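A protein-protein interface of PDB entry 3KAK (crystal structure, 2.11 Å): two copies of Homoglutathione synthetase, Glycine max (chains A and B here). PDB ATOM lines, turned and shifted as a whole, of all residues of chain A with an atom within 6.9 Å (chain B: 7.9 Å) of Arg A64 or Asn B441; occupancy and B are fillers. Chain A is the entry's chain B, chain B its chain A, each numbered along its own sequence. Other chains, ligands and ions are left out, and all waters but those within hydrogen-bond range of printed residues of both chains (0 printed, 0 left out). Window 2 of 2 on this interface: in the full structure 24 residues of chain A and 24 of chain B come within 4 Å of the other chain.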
ATOM      1  N   ASP A  59       3.811  18.454 -17.789  1.00  0.00           N
ATOM      2  CA  ASP A  59       2.833  17.993 -16.855  1.00  0.00           C
ATOM      3  C   ASP A  59       1.899  17.177 -17.728  1.00  0.00           C
ATOM      4  O   ASP A  59       1.385  17.734 -18.697  1.00  0.00           O
ATOM      5  CB  ASP A  59       2.143  19.211 -16.223  1.00  0.00           C
ATOM      6  CG  ASP A  59       1.221  18.861 -15.048  1.00  0.00           C
ATOM      7  OD1 ASP A  59       0.537  17.834 -15.078  1.00  0.00           O
ATOM      8  OD2 ASP A  59       1.182  19.664 -14.109  1.00  0.00           O
ATOM      9  N   SER A  61      -1.175  16.263 -16.893  1.00  0.00           N
ATOM     10  CA  SER A  61      -2.336  17.154 -16.904  1.00  0.00           C
ATOM     11  C   SER A  61      -2.467  18.206 -18.025  1.00  0.00           C
ATOM     12  O   SER A  61      -3.591  18.661 -18.288  1.00  0.00           O
ATOM     13  CB  SER A  61      -2.416  17.941 -15.584  1.00  0.00           C
ATOM     14  OG  SER A  61      -2.967  19.265 -15.818  1.00  0.00           O
ATOM     15  N   VAL A  62      -1.359  18.661 -18.619  1.00  0.00           N
ATOM     16  CA  VAL A  62      -1.399  19.642 -19.722  1.00  0.00           C
ATOM     17  C   VAL A  62      -1.096  18.963 -21.123  1.00  0.00           C
ATOM     18  O   VAL A  62       0.065  18.653 -21.479  1.00  0.00           O
ATOM     19  CB  VAL A  62      -0.470  20.850 -19.375  1.00  0.00           C
ATOM     20  CG1 VAL A  62      -0.501  21.962 -20.433  1.00  0.00           C
ATOM     21  CG2 VAL A  62      -0.797  21.417 -17.963  1.00  0.00           C
ATOM     22  N   GLN A  63      -2.162  18.721 -21.896  1.00  0.00           N
ATOM     23  CA  GLN A  63      -2.142  17.953 -23.190  1.00  0.00           C
ATOM     24  C   GLN A  63      -1.140  18.360 -24.321  1.00  0.00           C
ATOM     25  O   GLN A  63      -0.764  17.472 -25.129  1.00  0.00           O
ATOM     26  CB  GLN A  63      -3.557  17.861 -23.825  1.00  0.00           C
ATOM     27  CG  GLN A  63      -4.005  19.248 -24.308  1.00  0.00           C
ATOM     28  CD  GLN A  63      -3.563  20.325 -23.298  1.00  0.00           C
ATOM     29  OE1 GLN A  63      -2.499  20.946 -23.446  1.00  0.00           O
ATOM     30  NE2 GLN A  63      -4.347  20.482 -22.210  1.00  0.00           N
ATOM     31  N   ARG A  64      -0.760  19.655 -24.423  1.00  0.00           N
ATOM     32  CA  ARG A  64       0.274  20.129 -25.398  1.00  0.00           C
ATOM     33  C   ARG A  64       1.695  19.805 -24.881  1.00  0.00           C
ATOM     34  O   ARG A  64       2.670  19.777 -25.616  1.00  0.00           O
ATOM     35  CB  ARG A  64       0.202  21.614 -25.563  1.00  0.00           C
ATOM     36  CG  ARG A  64      -0.645  22.122 -26.667  1.00  0.00           C
ATOM     37  CD  ARG A  64      -1.229  23.534 -26.285  1.00  0.00           C
ATOM     38  NE  ARG A  64      -0.466  24.649 -26.851  1.00  0.00           N
ATOM     39  CZ  ARG A  64       0.027  25.670 -26.145  1.00  0.00           C
ATOM     40  NH1 ARG A  64      -0.191  25.761 -24.837  1.00  0.00           N
ATOM     41  NH2 ARG A  64       0.754  26.594 -26.767  1.00  0.00           N
ATOM     42  N   SER A  65       1.794  19.534 -23.601  1.00  0.00           N
ATOM     43  CA  SER A  65       3.094  19.536 -22.932  1.00  0.00           C
ATOM     44  C   SER A  65       4.106  18.446 -23.396  1.00  0.00           C
ATOM     45  O   SER A  65       5.212  18.438 -22.984  1.00  0.00           O
ATOM     46  CB  SER A  65       2.913  19.559 -21.427  1.00  0.00           C
ATOM     47  OG  SER A  65       2.849  18.260 -20.908  1.00  0.00           O
ATOM     48  N   GLY A  66       3.725  17.564 -24.272  1.00  0.00           N
ATOM     49  CA  GLY A  66       4.629  16.510 -24.678  1.00  0.00           C
ATOM     50  C   GLY A  66       5.095  16.699 -26.114  1.00  0.00           C
ATOM     51  O   GLY A  66       5.868  15.857 -26.636  1.00  0.00           O
ATOM     52  N   ARG A  67       4.684  17.853 -26.692  1.00  0.00           N
ATOM     53  CA  ARG A  67       4.914  18.239 -28.069  1.00  0.00           C
ATOM     54  C   ARG A  67       5.405  19.685 -28.121  1.00  0.00           C
ATOM     55  O   ARG A  67       6.323  20.012 -28.855  1.00  0.00           O
ATOM     56  CB  ARG A  67       3.574  18.230 -28.837  1.00  0.00           C
ATOM     57  CG  ARG A  67       2.823  16.891 -29.069  1.00  0.00           C
ATOM     58  CD  ARG A  67       1.719  17.068 -30.143  1.00  0.00           C
ATOM     59  NE  ARG A  67       0.995  18.342 -29.955  1.00  0.00           N
ATOM     60  CZ  ARG A  67      -0.025  18.511 -29.106  1.00  0.00           C
ATOM     61  NH1 ARG A  67      -0.459  17.455 -28.364  1.00  0.00           N
ATOM     62  NH2 ARG A  67      -0.615  19.727 -28.988  1.00  0.00           N
ATOM     63  N   VAL A  68       4.726  20.581 -27.398  1.00  0.00           N
ATOM     64  CA  VAL A  68       5.136  21.968 -27.285  1.00  0.00           C
ATOM     65  C   VAL A  68       6.168  22.216 -26.101  1.00  0.00           C
ATOM     66  O   VAL A  68       5.881  22.011 -24.906  1.00  0.00           O
ATOM     67  CB  VAL A  68       3.879  22.932 -27.341  1.00  0.00           C
ATOM     68  CG1 VAL A  68       4.263  24.364 -27.298  1.00  0.00           C
ATOM     69  CG2 VAL A  68       3.069  22.696 -28.650  1.00  0.00           C
ATOM     70  N   PRO A  69       7.386  22.659 -26.449  1.00  0.00           N
ATOM     71  CA  PRO A  69       8.380  22.904 -25.366  1.00  0.00           C
ATOM     72  C   PRO A  69       7.998  24.183 -24.597  1.00  0.00           C
ATOM     73  O   PRO A  69       7.202  24.968 -25.099  1.00  0.00           O
ATOM     74  CB  PRO A  69       9.714  22.960 -26.099  1.00  0.00           C
ATOM     75  CG  PRO A  69       9.347  23.218 -27.703  1.00  0.00           C
ATOM     76  CD  PRO A  69       7.850  22.985 -27.829  1.00  0.00           C
ATOM     77  N   VAL A  71       5.912  24.915 -22.251  1.00  0.00           N
ATOM     78  CA  VAL A  71       4.514  25.103 -21.700  1.00  0.00           C
ATOM     79  C   VAL A  71       4.162  23.943 -20.823  1.00  0.00           C
ATOM     80  O   VAL A  71       4.610  22.799 -21.065  1.00  0.00           O
ATOM     81  CB  VAL A  71       3.391  25.354 -22.816  1.00  0.00           C
ATOM     82  CG1 VAL A  71       3.913  26.299 -23.939  1.00  0.00           C
ATOM     83  CG2 VAL A  71       2.940  24.071 -23.482  1.00  0.00           C
ATOM     84  N   GLY A  72       3.453  24.213 -19.739  1.00  0.00           N
ATOM     85  CA  GLY A  72       2.915  23.101 -18.943  1.00  0.00           C
ATOM     86  C   GLY A  72       3.977  22.328 -18.183  1.00  0.00           C
ATOM     87  O   GLY A  72       3.882  21.151 -17.993  1.00  0.00           O
ATOM     88  N   GLU A 240       4.978  11.632 -28.424  1.00  0.00           N
ATOM     89  CA  GLU A 240       4.659  12.343 -27.212  1.00  0.00           C
ATOM     90  C   GLU A 240       5.846  12.106 -26.313  1.00  0.00           C
ATOM     91  O   GLU A 240       6.156  10.902 -25.975  1.00  0.00           O
ATOM     92  CB  GLU A 240       3.479  11.685 -26.531  1.00  0.00           C
ATOM     93  CG  GLU A 240       2.575  12.652 -25.970  1.00  0.00           C
ATOM     94  CD  GLU A 240       1.488  12.989 -26.937  1.00  0.00           C
ATOM     95  OE1 GLU A 240       0.431  12.385 -26.749  1.00  0.00           O
ATOM     96  OE2 GLU A 240       1.676  13.817 -27.859  1.00  0.00           O
ATOM     97  N   MET A 244      11.165  15.498 -22.819  1.00  0.00           N
ATOM     98  CA  MET A 244      11.958  15.927 -23.946  1.00  0.00           C
ATOM     99  C   MET A 244      13.204  16.671 -23.554  1.00  0.00           C
ATOM    100  O   MET A 244      14.142  16.788 -24.385  1.00  0.00           O
ATOM    101  CB  MET A 244      11.145  16.803 -24.896  1.00  0.00           C
ATOM    102  CG  MET A 244      10.559  18.088 -24.232  1.00  0.00           C
ATOM    103  SD  MET A 244       9.849  19.158 -25.483  1.00  0.00           S
ATOM    104  CE  MET A 244       8.163  18.672 -25.427  1.00  0.00           C
ATOM    105  N   VAL B  43      11.286  29.313 -33.436  1.00  0.00           N
ATOM    106  CA  VAL B  43      10.409  29.443 -32.295  1.00  0.00           C
ATOM    107  C   VAL B  43      10.515  28.232 -31.445  1.00  0.00           C
ATOM    108  O   VAL B  43      10.669  28.344 -30.173  1.00  0.00           O
ATOM    109  CB  VAL B  43       8.877  29.688 -32.739  1.00  0.00           C
ATOM    110  CG1 VAL B  43       7.871  29.249 -31.648  1.00  0.00           C
ATOM    111  CG2 VAL B  43       8.646  31.120 -33.238  1.00  0.00           C
ATOM    112  N   LEU B  47      11.871  27.990 -27.664  1.00  0.00           N
ATOM    113  CA  LEU B  47      11.054  27.451 -26.601  1.00  0.00           C
ATOM    114  C   LEU B  47      11.802  26.368 -25.779  1.00  0.00           C
ATOM    115  O   LEU B  47      11.695  26.262 -24.529  1.00  0.00           O
ATOM    116  CB  LEU B  47       9.793  26.893 -27.235  1.00  0.00           C
ATOM    117  CG  LEU B  47       8.823  27.966 -27.752  1.00  0.00           C
ATOM    118  CD1 LEU B  47       7.554  27.359 -28.383  1.00  0.00           C
ATOM    119  CD2 LEU B  47       8.430  28.857 -26.556  1.00  0.00           C
ATOM    120  N   ASP B  59       2.759  30.548 -14.720  1.00  0.00           N
ATOM    121  CA  ASP B  59       1.577  30.863 -15.544  1.00  0.00           C
ATOM    122  C   ASP B  59       0.567  31.635 -14.705  1.00  0.00           C
ATOM    123  O   ASP B  59       0.167  31.132 -13.672  1.00  0.00           O
ATOM    124  CB  ASP B  59       0.958  29.541 -16.046  1.00  0.00           C
ATOM    125  CG  ASP B  59       0.113  29.715 -17.292  1.00  0.00           C
ATOM    126  OD1 ASP B  59      -0.635  30.742 -17.426  1.00  0.00           O
ATOM    127  OD2 ASP B  59       0.230  28.844 -18.167  1.00  0.00           O
ATOM    128  N   VAL B  74       5.877  28.377 -17.122  1.00  0.00           N
ATOM    129  CA  VAL B  74       5.692  28.719 -18.540  1.00  0.00           C
ATOM    130  C   VAL B  74       6.844  29.649 -19.004  1.00  0.00           C
ATOM    131  O   VAL B  74       7.434  30.329 -18.160  1.00  0.00           O
ATOM    132  CB  VAL B  74       4.222  29.186 -18.861  1.00  0.00           C
ATOM    133  CG1 VAL B  74       3.909  30.606 -18.326  1.00  0.00           C
ATOM    134  CG2 VAL B  74       3.902  29.084 -20.363  1.00  0.00           C
ATOM    135  N   HIS B  75       7.204  29.632 -20.293  1.00  0.00           N
ATOM    136  CA  HIS B  75       8.302  30.470 -20.765  1.00  0.00           C
ATOM    137  C   HIS B  75       7.839  31.885 -20.605  1.00  0.00           C
ATOM    138  O   HIS B  75       6.636  32.099 -20.704  1.00  0.00           O
ATOM    139  CB  HIS B  75       8.675  30.200 -22.255  1.00  0.00           C
ATOM    140  CG  HIS B  75       7.558  30.457 -23.231  1.00  0.00           C
ATOM    141  ND1 HIS B  75       7.450  31.628 -23.959  1.00  0.00           N
ATOM    142  CD2 HIS B  75       6.513  29.669 -23.619  1.00  0.00           C
ATOM    143  CE1 HIS B  75       6.373  31.559 -24.738  1.00  0.00           C
ATOM    144  NE2 HIS B  75       5.770  30.389 -24.528  1.00  0.00           N
ATOM    145  N   LEU B  78       7.850  36.558 -25.207  1.00  0.00           N
ATOM    146  CA  LEU B  78       9.121  36.937 -25.766  1.00  0.00           C
ATOM    147  C   LEU B  78       9.084  37.342 -27.244  1.00  0.00           C
ATOM    148  O   LEU B  78       8.225  36.924 -28.007  1.00  0.00           O
ATOM    149  CB  LEU B  78      10.224  35.873 -25.391  1.00  0.00           C
ATOM    150  CG  LEU B  78      10.203  34.571 -26.203  1.00  0.00           C
ATOM    151  CD1 LEU B  78      11.055  34.685 -27.478  1.00  0.00           C
ATOM    152  CD2 LEU B  78      10.620  33.366 -25.414  1.00  0.00           C
ATOM    153  N   ILE B 435       8.287  39.048 -34.215  1.00  0.00           N
ATOM    154  CA  ILE B 435       7.581  37.773 -33.831  1.00  0.00           C
ATOM    155  C   ILE B 435       7.563  37.555 -32.315  1.00  0.00           C
ATOM    156  O   ILE B 435       8.590  37.557 -31.654  1.00  0.00           O
ATOM    157  CB  ILE B 435       8.174  36.489 -34.491  1.00  0.00           C
ATOM    158  CG1 ILE B 435       8.610  36.751 -35.953  1.00  0.00           C
ATOM    159  CG2 ILE B 435       7.173  35.309 -34.335  1.00  0.00           C
ATOM    160  CD1 ILE B 435       7.446  37.250 -36.928  1.00  0.00           C
ATOM    161  N   LEU B 436       6.369  37.304 -31.817  1.00  0.00           N
ATOM    162  CA  LEU B 436       5.991  37.401 -30.433  1.00  0.00           C
ATOM    163  C   LEU B 436       5.559  35.997 -30.096  1.00  0.00           C
ATOM    164  O   LEU B 436       4.690  35.447 -30.764  1.00  0.00           O
ATOM    165  CB  LEU B 436       4.823  38.411 -30.266  1.00  0.00           C
ATOM    166  CG  LEU B 436       5.111  39.770 -31.006  1.00  0.00           C
ATOM    167  CD1 LEU B 436       3.996  40.724 -31.085  1.00  0.00           C
ATOM    168  CD2 LEU B 436       6.365  40.519 -30.459  1.00  0.00           C
ATOM    169  N   VAL B 437       6.147  35.425 -29.047  1.00  0.00           N
ATOM    170  CA  VAL B 437       5.956  34.034 -28.709  1.00  0.00           C
ATOM    171  C   VAL B 437       5.318  34.039 -27.319  1.00  0.00           C
ATOM    172  O   VAL B 437       5.885  34.574 -26.355  1.00  0.00           O
ATOM    173  CB  VAL B 437       7.333  33.261 -28.708  1.00  0.00           C
ATOM    174  CG1 VAL B 437       7.144  31.686 -28.452  1.00  0.00           C
ATOM    175  CG2 VAL B 437       8.111  33.491 -29.987  1.00  0.00           C
ATOM    176  N   ARG B 438       4.152  33.439 -27.186  1.00  0.00           N
ATOM    177  CA  ARG B 438       3.478  33.524 -25.928  1.00  0.00           C
ATOM    178  C   ARG B 438       2.693  32.257 -25.671  1.00  0.00           C
ATOM    179  O   ARG B 438       1.923  31.809 -26.552  1.00  0.00           O
ATOM    180  CB  ARG B 438       2.537  34.726 -26.013  1.00  0.00           C
ATOM    181  CG  ARG B 438       1.987  35.220 -24.719  1.00  0.00           C
ATOM    182  CD  ARG B 438       0.998  36.328 -25.050  1.00  0.00           C
ATOM    183  NE  ARG B 438       1.673  37.628 -25.047  1.00  0.00           N
ATOM    184  CZ  ARG B 438       2.025  38.324 -23.939  1.00  0.00           C
ATOM    185  NH1 ARG B 438       1.778  37.878 -22.681  1.00  0.00           N
ATOM    186  NH2 ARG B 438       2.638  39.495 -24.091  1.00  0.00           N
ATOM    187  N   ASP B 439       2.883  31.676 -24.491  1.00  0.00           N
ATOM    188  CA  ASP B 439       2.347  30.332 -24.143  1.00  0.00           C
ATOM    189  C   ASP B 439       2.496  29.365 -25.323  1.00  0.00           C
ATOM    190  O   ASP B 439       1.560  28.675 -25.714  1.00  0.00           O
ATOM    191  CB  ASP B 439       0.872  30.444 -23.618  1.00  0.00           C
ATOM    192  CG  ASP B 439       0.370  29.184 -22.814  1.00  0.00           C
ATOM    193  OD1 ASP B 439      -0.848  29.003 -22.806  1.00  0.00           O
ATOM    194  OD2 ASP B 439       1.123  28.378 -22.187  1.00  0.00           O
ATOM    195  N   GLY B 440       3.704  29.264 -25.861  1.00  0.00           N
ATOM    196  CA  GLY B 440       4.029  28.304 -26.876  1.00  0.00           C
ATOM    197  C   GLY B 440       3.595  28.586 -28.299  1.00  0.00           C
ATOM    198  O   GLY B 440       3.840  27.747 -29.197  1.00  0.00           O
ATOM    199  N   ASN B 441       2.969  29.747 -28.538  1.00  0.00           N
ATOM    200  CA  ASN B 441       2.363  30.100 -29.819  1.00  0.00           C
ATOM    201  C   ASN B 441       2.912  31.462 -30.288  1.00  0.00           C
ATOM    202  O   ASN B 441       2.999  32.412 -29.533  1.00  0.00           O
ATOM    203  CB  ASN B 441       0.851  30.367 -29.651  1.00  0.00           C
ATOM    204  CG  ASN B 441      -0.005  29.114 -29.605  1.00  0.00           C
ATOM    205  OD1 ASN B 441      -0.071  28.355 -30.560  1.00  0.00           O
ATOM    206  ND2 ASN B 441      -0.747  28.963 -28.525  1.00  0.00           N
ATOM    207  N   TRP B 442       3.186  31.582 -31.559  1.00  0.00           N
ATOM    208  CA  TRP B 442       3.687  32.833 -32.048  1.00  0.00           C
ATOM    209  C   TRP B 442       2.647  33.522 -32.889  1.00  0.00           C
ATOM    210  O   TRP B 442       1.572  32.941 -33.205  1.00  0.00           O
ATOM    211  CB  TRP B 442       4.944  32.595 -32.819  1.00  0.00           C
ATOM    212  CG  TRP B 442       4.786  31.445 -33.739  1.00  0.00           C
ATOM    213  CD1 TRP B 442       4.513  30.154 -33.395  1.00  0.00           C
ATOM    214  CD2 TRP B 442       4.932  31.462 -35.148  1.00  0.00           C
ATOM    215  NE1 TRP B 442       4.458  29.379 -34.507  1.00  0.00           N
ATOM    216  CE2 TRP B 442       4.708  30.161 -35.602  1.00  0.00           C
ATOM    217  CE3 TRP B 442       5.213  32.465 -36.079  1.00  0.00           C
ATOM    218  CZ2 TRP B 442       4.754  29.820 -36.960  1.00  0.00           C
ATOM    219  CZ3 TRP B 442       5.260  32.131 -37.416  1.00  0.00           C
ATOM    220  CH2 TRP B 442       5.038  30.820 -37.844  1.00  0.00           C
ATOM    221  N   ASP B 443       2.938  34.775 -33.211  1.00  0.00           N
ATOM    222  CA  ASP B 443       2.036  35.599 -33.953  1.00  0.00           C
ATOM    223  C   ASP B 443       2.913  36.782 -34.329  1.00  0.00           C
ATOM    224  O   ASP B 443       3.979  36.923 -33.770  1.00  0.00           O
ATOM    225  CB  ASP B 443       0.850  36.030 -33.093  1.00  0.00           C
ATOM    226  CG  ASP B 443      -0.434  36.299 -33.917  1.00  0.00           C
ATOM    227  OD1 ASP B 443      -0.376  36.299 -35.176  1.00  0.00           O
ATOM    228  OD2 ASP B 443      -1.504  36.497 -33.286  1.00  0.00           O
ATOM    229  N   THR B 444       2.478  37.608 -35.289  1.00  0.00           N
ATOM    230  CA  THR B 444       3.295  38.695 -35.727  1.00  0.00           C
ATOM    231  C   THR B 444       2.677  39.976 -35.208  1.00  0.00           C
ATOM    232  O   THR B 444       1.470  40.028 -34.889  1.00  0.00           O
ATOM    233  CB  THR B 444       3.513  38.660 -37.251  1.00  0.00           C
ATOM    234  OG1 THR B 444       2.327  39.069 -37.954  1.00  0.00           O
ATOM    235  CG2 THR B 444       3.918  37.230 -37.701  1.00  0.00           C
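NH2 of Arg A64 touches CA of Gly B440, at 3.7 Å. Val A68 touches Gly B440 (CG1 to O, 3.9 Å). CG of Pro A69 touches CB of Leu B47, 3.7 Å away. CG1 of Val A71 touches C of Asp B439, at 3.7 Å. CG1 of Val A71 touches N of Gly B440, 3.5 Å away.
Hydrophobic or aromatic side chains of chain A that line the printed part of chain B: Val A68, Pro A69 and Val A71. Of the 16 printed residues of chain B, 4 touch a printed residue of chain A. Hydrophobic or aromatic side chains of chain B that line the printed part of chain A: Leu B47. Among the printed residues, Asp or Glu carboxylates within 4 Å of a Lys or Arg side-chain nitrogen of the other chain: Arg A64 with Asp B439.
Arg A64 touches just these residues of chain B: Asp B439, Gly B440 and Asn B441. Printed residues of chain A within 4 Å of Asn B441: Arg A64. Of chain A, only Arg A64 (3.7 Å), Val A68 (3.9 Å) and Val A71 (3.5 Å) come within 4 Å of Gly B440. Printed residues of chain B within 4 Å of Val A71: Asp B439 and Gly B440. Of the printed residues of chain B, Val A68 touches Gly B440. Of the printed residues of chain A, Asp B439 touches Arg A64 and Val A71. Asp B443 touches none of the printed residues of chain A. Ser A61 touches none of the printed residues of chain B. The nearest printed residue of chain A that does not touch Leu B47 is Val A68 (4.6 Å).
NH1 of Arg A64 is in salt-bridge range of OD1 of Asp B439, at 3.9 Å. NH2 of Arg A64 lies close to ND2 of Asn B441, 3.3 Å away.
A ring nitrogen (NE2) of His B75 is in hydrogen-bond range of the backbone NH of Asp B439. A ring nitrogen (NE2) of His B75 sits at hydrogen-bond distance from the backbone NH (N) of Gly B440.
1 position is printed for both chains. Of the 7 pairs that touch across the chains among the printed residues, none has its exchanged pair printed and touching as well.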
